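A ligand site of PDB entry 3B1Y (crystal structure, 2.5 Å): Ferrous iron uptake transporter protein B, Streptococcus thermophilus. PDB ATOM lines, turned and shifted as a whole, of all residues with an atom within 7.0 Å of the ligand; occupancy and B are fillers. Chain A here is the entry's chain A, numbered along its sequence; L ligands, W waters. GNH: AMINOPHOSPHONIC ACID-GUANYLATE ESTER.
O2B of the ligand lies within hydrogen-bond range of N of Thr 17, 2.8 Å away. O2B of the ligand sits at hydrogen-bond distance from OG1 of Thr 17 (2.6 Å). N1 of the ligand is in hydrogen-bond range of OD1 of Asp 118 (2.6 Å). N of Ser 18 sits at hydrogen-bond distance from O1A of the ligand. O1A of the ligand lies within hydrogen-bond range of OG of Ser 18 (2.8 Å). An oxygen (O6) of the ligand is in hydrogen-bond range of the backbone NH (N) of Ala 145 (3.0 Å). The side-chain amide nitrogen (ND2) of Asn 115 is in hydrogen-bond range of a nitrogen (N7) of the ligand (3.0 Å). An oxygen (O1B) of the ligand sits at hydrogen-bond distance from the backbone NH of Asn 13 (3.2 Å). N of Lys 16 lies within hydrogen-bond range of O1B of the ligand (3.1 Å). The backbone NH (N) of Gly 15 is in hydrogen-bond range of an oxygen (O3A) of the ligand, 3.2 Å away. O1B of the ligand lies within hydrogen-bond range of N of Ser 14, at 3.2 Å. An oxygen (O6) of the ligand is in hydrogen-bond range of the backbone NH (N) of Met 116, at 3.3 Å.
The side-chain carboxylate of Asp 118 sits at hydrogen-bond distance from the side-chain hydroxyl of Ser 144, 2.6 Å away. The backbone carbonyl oxygen of Ala 145 sits at hydrogen-bond distance from the side-chain amide nitrogen of Gln 148, 2.8 Å away. The side-chain amide nitrogen of Asn 115 is in hydrogen-bond range of the backbone carbonyl oxygen of Ser 14, at 2.8 Å. The side-chain amide oxygen (OD1) of Asn 115 is in hydrogen-bond range of the side-chain hydroxyl (OG1) of Thr 143 (3.1 Å). The side-chain hydroxyl (OG) of Ser 14 sits at hydrogen-bond distance from the backbone carbonyl oxygen (O) of Asn 11. The backbone carbonyl oxygen (O) of Thr 143 lies within hydrogen-bond range of the backbone NH (N) of Met 116 (3.4 Å). The backbone NH (N) of Lys 147 sits at hydrogen-bond distance from the side-chain hydroxyl (OG) of Ser 144 (3.2 Å). The side-chain amide nitrogen (NE2) of Gln 148 lies within hydrogen-bond range of the backbone carbonyl oxygen (O) of Leu 146 (2.7 Å).
Residues that only touch the ligand: Val 119 (3.2 Å), Ser 144 (3.5 Å), Leu 146 (3.6 Å), Asn 11 (3.9 Å) and Pro 12 (3.99 Å). Hydrophobic or aromatic side chains that line the ligand: Met 116, Val 119, Ala 145 and Leu 146. Of the 26 residues printed, 15 come within 4 Å of the ligand. Along chain A the residues within 4 Å of the ligand span positions 11 to 146. The nearest printed residue that does not touch the ligand is Thr 143 (4.5 Å).
Water W1 bridges O1B of the ligand and O of Asn 11.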
ATOM      1  N   GLY A  10      -4.084 -22.348  27.430  1.00  0.00           N
ATOM      2  CA  GLY A  10      -4.641 -23.654  27.758  1.00  0.00           C
ATOM      3  C   GLY A  10      -3.528 -24.552  28.229  1.00  0.00           C
ATOM      4  O   GLY A  10      -2.369 -24.115  28.259  1.00  0.00           O
ATOM      5  N   ASN A  11      -3.855 -25.779  28.585  1.00  0.00           N
ATOM      6  CA  ASN A  11      -2.849 -26.755  28.974  1.00  0.00           C
ATOM      7  C   ASN A  11      -1.858 -27.037  27.850  1.00  0.00           C
ATOM      8  O   ASN A  11      -2.229 -26.908  26.683  1.00  0.00           O
ATOM      9  CB  ASN A  11      -3.476 -28.112  29.341  1.00  0.00           C
ATOM     10  CG  ASN A  11      -4.177 -28.130  30.695  1.00  0.00           C
ATOM     11  OD1 ASN A  11      -4.651 -29.188  31.124  1.00  0.00           O
ATOM     12  ND2 ASN A  11      -4.240 -26.983  31.369  1.00  0.00           N
ATOM     13  N   PRO A  12      -0.618 -27.417  28.191  1.00  0.00           N
ATOM     14  CA  PRO A  12       0.324 -27.910  27.195  1.00  0.00           C
ATOM     15  C   PRO A  12      -0.261 -29.073  26.394  1.00  0.00           C
ATOM     16  O   PRO A  12      -1.024 -29.867  26.918  1.00  0.00           O
ATOM     17  CB  PRO A  12       1.488 -28.406  28.038  1.00  0.00           C
ATOM     18  CG  PRO A  12       1.504 -27.490  29.169  1.00  0.00           C
ATOM     19  CD  PRO A  12       0.044 -27.307  29.507  1.00  0.00           C
ATOM     20  N   ASN A  13       0.106 -29.140  25.123  1.00  0.00           N
ATOM     21  CA  ASN A  13      -0.379 -30.174  24.199  1.00  0.00           C
ATOM     22  C   ASN A  13      -1.915 -30.281  24.024  1.00  0.00           C
ATOM     23  O   ASN A  13      -2.455 -31.354  23.820  1.00  0.00           O
ATOM     24  CB  ASN A  13       0.251 -31.527  24.551  1.00  0.00           C
ATOM     25  CG  ASN A  13       0.648 -32.300  23.306  1.00  0.00           C
ATOM     26  OD1 ASN A  13       0.077 -33.336  22.976  1.00  0.00           O
ATOM     27  ND2 ASN A  13       1.640 -31.762  22.583  1.00  0.00           N
ATOM     28  N   SER A  14      -2.590 -29.144  24.105  1.00  0.00           N
ATOM     29  CA  SER A  14      -4.007 -29.052  23.820  1.00  0.00           C
ATOM     30  C   SER A  14      -4.242 -28.626  22.357  1.00  0.00           C
ATOM     31  O   SER A  14      -5.383 -28.666  21.880  1.00  0.00           O
ATOM     32  CB  SER A  14      -4.675 -28.070  24.799  1.00  0.00           C
ATOM     33  OG  SER A  14      -4.064 -26.799  24.734  1.00  0.00           O
ATOM     34  N   GLY A  15      -3.168 -28.237  21.668  1.00  0.00           N
ATOM     35  CA  GLY A  15      -3.197 -27.842  20.250  1.00  0.00           C
ATOM     36  C   GLY A  15      -3.171 -26.340  20.044  1.00  0.00           C
ATOM     37  O   GLY A  15      -3.670 -25.829  19.044  1.00  0.00           O
ATOM     38  N   LYS A  16      -2.555 -25.648  21.001  1.00  0.00           N
ATOM     39  CA  LYS A  16      -2.584 -24.196  21.044  1.00  0.00           C
ATOM     40  C   LYS A  16      -1.725 -23.571  19.948  1.00  0.00           C
ATOM     41  O   LYS A  16      -2.170 -22.679  19.236  1.00  0.00           O
ATOM     42  CB  LYS A  16      -2.116 -23.727  22.420  1.00  0.00           C
ATOM     43  CG  LYS A  16      -2.701 -22.411  22.861  1.00  0.00           C
ATOM     44  CD  LYS A  16      -1.648 -21.427  23.257  1.00  0.00           C
ATOM     45  CE  LYS A  16      -0.739 -21.822  24.436  1.00  0.00           C
ATOM     46  NZ  LYS A  16       0.544 -21.071  24.282  1.00  0.00           N
ATOM     47  N   THR A  17      -0.493 -24.037  19.810  1.00  0.00           N
ATOM     48  CA  THR A  17       0.363 -23.611  18.717  1.00  0.00           C
ATOM     49  C   THR A  17      -0.349 -23.800  17.369  1.00  0.00           C
ATOM     50  O   THR A  17      -0.383 -22.875  16.558  1.00  0.00           O
ATOM     51  CB  THR A  17       1.700 -24.398  18.698  1.00  0.00           C
ATOM     52  OG1 THR A  17       2.355 -24.267  19.963  1.00  0.00           O
ATOM     53  CG2 THR A  17       2.603 -23.876  17.574  1.00  0.00           C
ATOM     54  N   SER A  18      -0.911 -25.009  17.166  1.00  0.00           N
ATOM     55  CA  SER A  18      -1.638 -25.368  15.946  1.00  0.00           C
ATOM     56  C   SER A  18      -2.784 -24.403  15.653  1.00  0.00           C
ATOM     57  O   SER A  18      -2.900 -23.926  14.525  1.00  0.00           O
ATOM     58  CB  SER A  18      -2.185 -26.793  16.020  1.00  0.00           C
ATOM     59  OG  SER A  18      -1.134 -27.736  16.161  1.00  0.00           O
ATOM     60  N   LEU A  19      -3.620 -24.130  16.659  1.00  0.00           N
ATOM     61  CA  LEU A  19      -4.701 -23.163  16.492  1.00  0.00           C
ATOM     62  C   LEU A  19      -4.157 -21.753  16.258  1.00  0.00           C
ATOM     63  O   LEU A  19      -4.642 -21.035  15.388  1.00  0.00           O
ATOM     64  CB  LEU A  19      -5.647 -23.130  17.699  1.00  0.00           C
ATOM     65  CG  LEU A  19      -6.579 -24.321  17.867  1.00  0.00           C
ATOM     66  CD1 LEU A  19      -7.331 -24.185  19.171  1.00  0.00           C
ATOM     67  CD2 LEU A  19      -7.540 -24.408  16.657  1.00  0.00           C
ATOM     68  N   PHE A  20      -3.152 -21.369  17.047  1.00  0.00           N
ATOM     69  CA  PHE A  20      -2.522 -20.057  16.934  1.00  0.00           C
ATOM     70  C   PHE A  20      -1.987 -19.795  15.515  1.00  0.00           C
ATOM     71  O   PHE A  20      -2.213 -18.716  14.969  1.00  0.00           O
ATOM     72  CB  PHE A  20      -1.372 -19.925  17.948  1.00  0.00           C
ATOM     73  CG  PHE A  20      -0.708 -18.589  17.912  1.00  0.00           C
ATOM     74  CD1 PHE A  20      -1.278 -17.495  18.572  1.00  0.00           C
ATOM     75  CD2 PHE A  20       0.502 -18.412  17.230  1.00  0.00           C
ATOM     76  CE1 PHE A  20      -0.649 -16.241  18.552  1.00  0.00           C
ATOM     77  CE2 PHE A  20       1.126 -17.179  17.198  1.00  0.00           C
ATOM     78  CZ  PHE A  20       0.543 -16.089  17.864  1.00  0.00           C
ATOM     79  N   ASN A  21      -1.299 -20.782  14.948  1.00  0.00           N
ATOM     80  CA  ASN A  21      -0.755 -20.687  13.587  1.00  0.00           C
ATOM     81  C   ASN A  21      -1.845 -20.606  12.520  1.00  0.00           C
ATOM     82  O   ASN A  21      -1.675 -19.851  11.561  1.00  0.00           O
ATOM     83  CB  ASN A  21       0.185 -21.864  13.278  1.00  0.00           C
ATOM     84  CG  ASN A  21       1.495 -21.801  14.047  1.00  0.00           C
ATOM     85  OD1 ASN A  21       1.872 -20.777  14.660  1.00  0.00           O
ATOM     86  ND2 ASN A  21       2.212 -22.908  14.028  1.00  0.00           N
ATOM     87  N   GLY A  58       1.604 -22.228  27.794  1.00  0.00           N
ATOM     88  CA  GLY A  58       0.757 -23.365  28.155  1.00  0.00           C
ATOM     89  C   GLY A  58       0.992 -23.680  29.603  1.00  0.00           C
ATOM     90  O   GLY A  58       2.133 -23.825  30.014  1.00  0.00           O
ATOM     91  N   VAL A  87      -8.007 -22.786  25.000  1.00  0.00           N
ATOM     92  CA  VAL A  87      -7.848 -24.013  24.216  1.00  0.00           C
ATOM     93  C   VAL A  87      -7.938 -25.199  25.185  1.00  0.00           C
ATOM     94  O   VAL A  87      -7.139 -25.282  26.121  1.00  0.00           O
ATOM     95  CB  VAL A  87      -6.534 -24.088  23.424  1.00  0.00           C
ATOM     96  CG1 VAL A  87      -6.466 -25.375  22.610  1.00  0.00           C
ATOM     97  CG2 VAL A  87      -6.417 -22.912  22.507  1.00  0.00           C
ATOM     98  N   LEU A 114     -12.963 -26.136  22.122  1.00  0.00           N
ATOM     99  CA  LEU A 114     -12.974 -27.521  22.581  1.00  0.00           C
ATOM    100  C   LEU A 114     -12.222 -28.286  21.503  1.00  0.00           C
ATOM    101  O   LEU A 114     -12.846 -28.858  20.593  1.00  0.00           O
ATOM    102  CB  LEU A 114     -14.417 -27.985  22.789  1.00  0.00           C
ATOM    103  CG  LEU A 114     -14.671 -29.396  23.361  1.00  0.00           C
ATOM    104  CD1 LEU A 114     -14.045 -29.585  24.760  1.00  0.00           C
ATOM    105  CD2 LEU A 114     -16.188 -29.699  23.350  1.00  0.00           C
ATOM    106  N   ASN A 115     -10.891 -28.274  21.599  1.00  0.00           N
ATOM    107  CA  ASN A 115     -10.021 -28.815  20.553  1.00  0.00           C
ATOM    108  C   ASN A 115      -9.885 -30.322  20.604  1.00  0.00           C
ATOM    109  O   ASN A 115     -10.230 -30.929  21.612  1.00  0.00           O
ATOM    110  CB  ASN A 115      -8.638 -28.162  20.603  1.00  0.00           C
ATOM    111  CG  ASN A 115      -7.879 -28.282  19.276  1.00  0.00           C
ATOM    112  OD1 ASN A 115      -8.438 -28.016  18.209  1.00  0.00           O
ATOM    113  ND2 ASN A 115      -6.626 -28.683  19.343  1.00  0.00           N
ATOM    114  N   MET A 116      -9.383 -30.886  19.510  1.00  0.00           N
ATOM    115  CA  MET A 116      -9.137 -32.312  19.333  1.00  0.00           C
ATOM    116  C   MET A 116     -10.444 -33.093  19.266  1.00  0.00           C
ATOM    117  O   MET A 116     -10.487 -34.255  19.665  1.00  0.00           O
ATOM    118  CB  MET A 116      -8.181 -32.874  20.402  1.00  0.00           C
ATOM    119  CG  MET A 116      -6.907 -32.058  20.549  1.00  0.00           C
ATOM    120  SD  MET A 116      -5.495 -33.027  21.124  1.00  0.00           S
ATOM    121  CE  MET A 116      -4.159 -31.830  20.993  1.00  0.00           C
ATOM    122  N   ILE A 117     -11.489 -32.446  18.751  1.00  0.00           N
ATOM    123  CA  ILE A 117     -12.814 -33.066  18.641  1.00  0.00           C
ATOM    124  C   ILE A 117     -12.772 -34.263  17.684  1.00  0.00           C
ATOM    125  O   ILE A 117     -13.512 -35.233  17.879  1.00  0.00           O
ATOM    126  CB  ILE A 117     -13.916 -32.033  18.233  1.00  0.00           C
ATOM    127  CG1 ILE A 117     -15.323 -32.521  18.624  1.00  0.00           C
ATOM    128  CG2 ILE A 117     -13.842 -31.695  16.740  1.00  0.00           C
ATOM    129  CD1 ILE A 117     -15.624 -32.421  20.118  1.00  0.00           C
ATOM    130  N   ASP A 118     -11.902 -34.196  16.661  1.00  0.00           N
ATOM    131  CA  ASP A 118     -11.696 -35.295  15.713  1.00  0.00           C
ATOM    132  C   ASP A 118     -11.240 -36.613  16.359  1.00  0.00           C
ATOM    133  O   ASP A 118     -11.675 -37.680  15.941  1.00  0.00           O
ATOM    134  CB  ASP A 118     -10.698 -34.895  14.620  1.00  0.00           C
ATOM    135  CG  ASP A 118      -9.304 -34.615  15.164  1.00  0.00           C
ATOM    136  OD1 ASP A 118      -9.097 -33.513  15.708  1.00  0.00           O
ATOM    137  OD2 ASP A 118      -8.428 -35.485  15.043  1.00  0.00           O
ATOM    138  N   VAL A 119     -10.382 -36.526  17.383  1.00  0.00           N
ATOM    139  CA  VAL A 119      -9.854 -37.694  18.096  1.00  0.00           C
ATOM    140  C   VAL A 119     -10.947 -38.315  18.962  1.00  0.00           C
ATOM    141  O   VAL A 119     -11.069 -39.537  19.015  1.00  0.00           O
ATOM    142  CB  VAL A 119      -8.657 -37.349  19.018  1.00  0.00           C
ATOM    143  CG1 VAL A 119      -8.146 -38.584  19.763  1.00  0.00           C
ATOM    144  CG2 VAL A 119      -7.510 -36.737  18.226  1.00  0.00           C
ATOM    145  N   THR A 143     -13.670 -27.598  17.992  1.00  0.00           N
ATOM    146  CA  THR A 143     -12.711 -27.310  16.936  1.00  0.00           C
ATOM    147  C   THR A 143     -11.786 -28.489  16.646  1.00  0.00           C
ATOM    148  O   THR A 143     -11.628 -29.396  17.474  1.00  0.00           O
ATOM    149  CB  THR A 143     -11.815 -26.085  17.284  1.00  0.00           C
ATOM    150  OG1 THR A 143     -11.064 -26.356  18.477  1.00  0.00           O
ATOM    151  CG2 THR A 143     -12.647 -24.835  17.514  1.00  0.00           C
ATOM    152  N   SER A 144     -11.196 -28.456  15.456  1.00  0.00           N
ATOM    153  CA  SER A 144     -10.129 -29.386  15.110  1.00  0.00           C
ATOM    154  C   SER A 144      -9.042 -28.642  14.337  1.00  0.00           C
ATOM    155  O   SER A 144      -9.268 -28.225  13.188  1.00  0.00           O
ATOM    156  CB  SER A 144     -10.622 -30.574  14.290  1.00  0.00           C
ATOM    157  OG  SER A 144      -9.552 -31.480  14.095  1.00  0.00           O
ATOM    158  N   ALA A 145      -7.870 -28.492  14.953  1.00  0.00           N
ATOM    159  CA  ALA A 145      -6.712 -27.861  14.307  1.00  0.00           C
ATOM    160  C   ALA A 145      -6.152 -28.746  13.196  1.00  0.00           C
ATOM    161  O   ALA A 145      -5.532 -28.245  12.264  1.00  0.00           O
ATOM    162  CB  ALA A 145      -5.641 -27.545  15.325  1.00  0.00           C
ATOM    163  N   LEU A 146      -6.378 -30.059  13.289  1.00  0.00           N
ATOM    164  CA  LEU A 146      -5.957 -31.044  12.292  1.00  0.00           C
ATOM    165  C   LEU A 146      -6.829 -30.932  11.046  1.00  0.00           C
ATOM    166  O   LEU A 146      -6.288 -30.776   9.960  1.00  0.00           O
ATOM    167  CB  LEU A 146      -6.032 -32.477  12.857  1.00  0.00           C
ATOM    168  CG  LEU A 146      -5.464 -33.622  12.007  1.00  0.00           C
ATOM    169  CD1 LEU A 146      -3.933 -33.603  11.918  1.00  0.00           C
ATOM    170  CD2 LEU A 146      -5.952 -34.977  12.531  1.00  0.00           C
ATOM    171  N   LYS A 147      -8.144 -30.994  11.207  1.00  0.00           N
ATOM    172  CA  LYS A 147      -9.082 -30.904  10.084  1.00  0.00           C
ATOM    173  C   LYS A 147      -9.464 -29.462   9.717  1.00  0.00           C
ATOM    174  O   LYS A 147     -10.170 -29.228   8.735  1.00  0.00           O
ATOM    175  CB  LYS A 147     -10.348 -31.715  10.403  1.00  0.00           C
ATOM    176  CG  LYS A 147     -10.141 -33.221  10.588  1.00  0.00           C
ATOM    177  CD  LYS A 147      -9.949 -33.881   9.229  1.00  0.00           C
ATOM    178  CE  LYS A 147      -9.732 -35.395   9.271  1.00  0.00           C
ATOM    179  NZ  LYS A 147      -9.461 -35.906   7.885  1.00  0.00           N
ATOM    180  N   GLN A 148      -8.990 -28.501  10.521  1.00  0.00           N
ATOM    181  CA  GLN A 148      -9.249 -27.069  10.339  1.00  0.00           C
ATOM    182  C   GLN A 148     -10.734 -26.706  10.434  1.00  0.00           C
ATOM    183  O   GLN A 148     -11.238 -25.904   9.646  1.00  0.00           O
ATOM    184  CB  GLN A 148      -8.603 -26.514   9.047  1.00  0.00           C
ATOM    185  CG  GLN A 148      -7.069 -26.488   9.060  1.00  0.00           C
ATOM    186  CD  GLN A 148      -6.415 -27.801   8.663  1.00  0.00           C
ATOM    187  OE1 GLN A 148      -6.765 -28.395   7.650  1.00  0.00           O
ATOM    188  NE2 GLN A 148      -5.457 -28.244   9.464  1.00  0.00           N
HETATM  189  N3B GNH L   1       1.702 -27.776  22.902  1.00  0.00           N
HETATM  190  PB  GNH L   1       0.400 -27.213  22.155  1.00  0.00           P
HETATM  191  O1B GNH L   1      -0.673 -26.839  23.108  1.00  0.00           O
HETATM  192  O2B GNH L   1       0.879 -25.966  21.274  1.00  0.00           O
HETATM  193  O3A GNH L   1      -0.063 -28.371  21.106  1.00  0.00           O
HETATM  194  PA  GNH L   1       0.398 -28.312  19.520  1.00  0.00           P
HETATM  195  O1A GNH L   1      -0.275 -27.211  18.758  1.00  0.00           O
HETATM  196  O2A GNH L   1       1.998 -28.184  19.527  1.00  0.00           O
HETATM  197  O5' GNH L   1       0.080 -29.732  18.934  1.00  0.00           O
HETATM  198  C5' GNH L   1       0.688 -30.898  19.502  1.00  0.00           C
HETATM  199  C4' GNH L   1       0.246 -32.113  18.662  1.00  0.00           C
HETATM  200  O4' GNH L   1      -1.182 -32.142  18.695  1.00  0.00           O
HETATM  201  C3' GNH L   1       0.660 -31.919  17.192  1.00  0.00           C
HETATM  202  O3' GNH L   1       0.985 -33.184  16.645  1.00  0.00           O
HETATM  203  C2' GNH L   1      -0.586 -31.400  16.511  1.00  0.00           C
HETATM  204  O2' GNH L   1      -0.643 -31.827  15.129  1.00  0.00           O
HETATM  205  C1' GNH L   1      -1.676 -32.114  17.359  1.00  0.00           C
HETATM  206  N9  GNH L   1      -3.001 -31.402  17.359  1.00  0.00           N
HETATM  207  C8  GNH L   1      -3.318 -30.134  17.626  1.00  0.00           C
HETATM  208  N7  GNH L   1      -4.617 -29.930  17.493  1.00  0.00           N
HETATM  209  C5  GNH L   1      -5.154 -31.086  17.136  1.00  0.00           C
HETATM  210  C6  GNH L   1      -6.454 -31.464  16.871  1.00  0.00           C
HETATM  211  O6  GNH L   1      -7.399 -30.677  16.933  1.00  0.00           O
HETATM  212  N1  GNH L   1      -6.699 -32.776  16.516  1.00  0.00           N
HETATM  213  C2  GNH L   1      -5.634 -33.702  16.435  1.00  0.00           C
HETATM  214  N2  GNH L   1      -5.867 -34.963  16.094  1.00  0.00           N
HETATM  215  N3  GNH L   1      -4.381 -33.300  16.707  1.00  0.00           N
HETATM  216  C4  GNH L   1      -4.139 -32.022  17.046  1.00  0.00           C
HETATM  217  O   HOH W   1      -0.695 -25.182  24.899  1.00  0.00           O
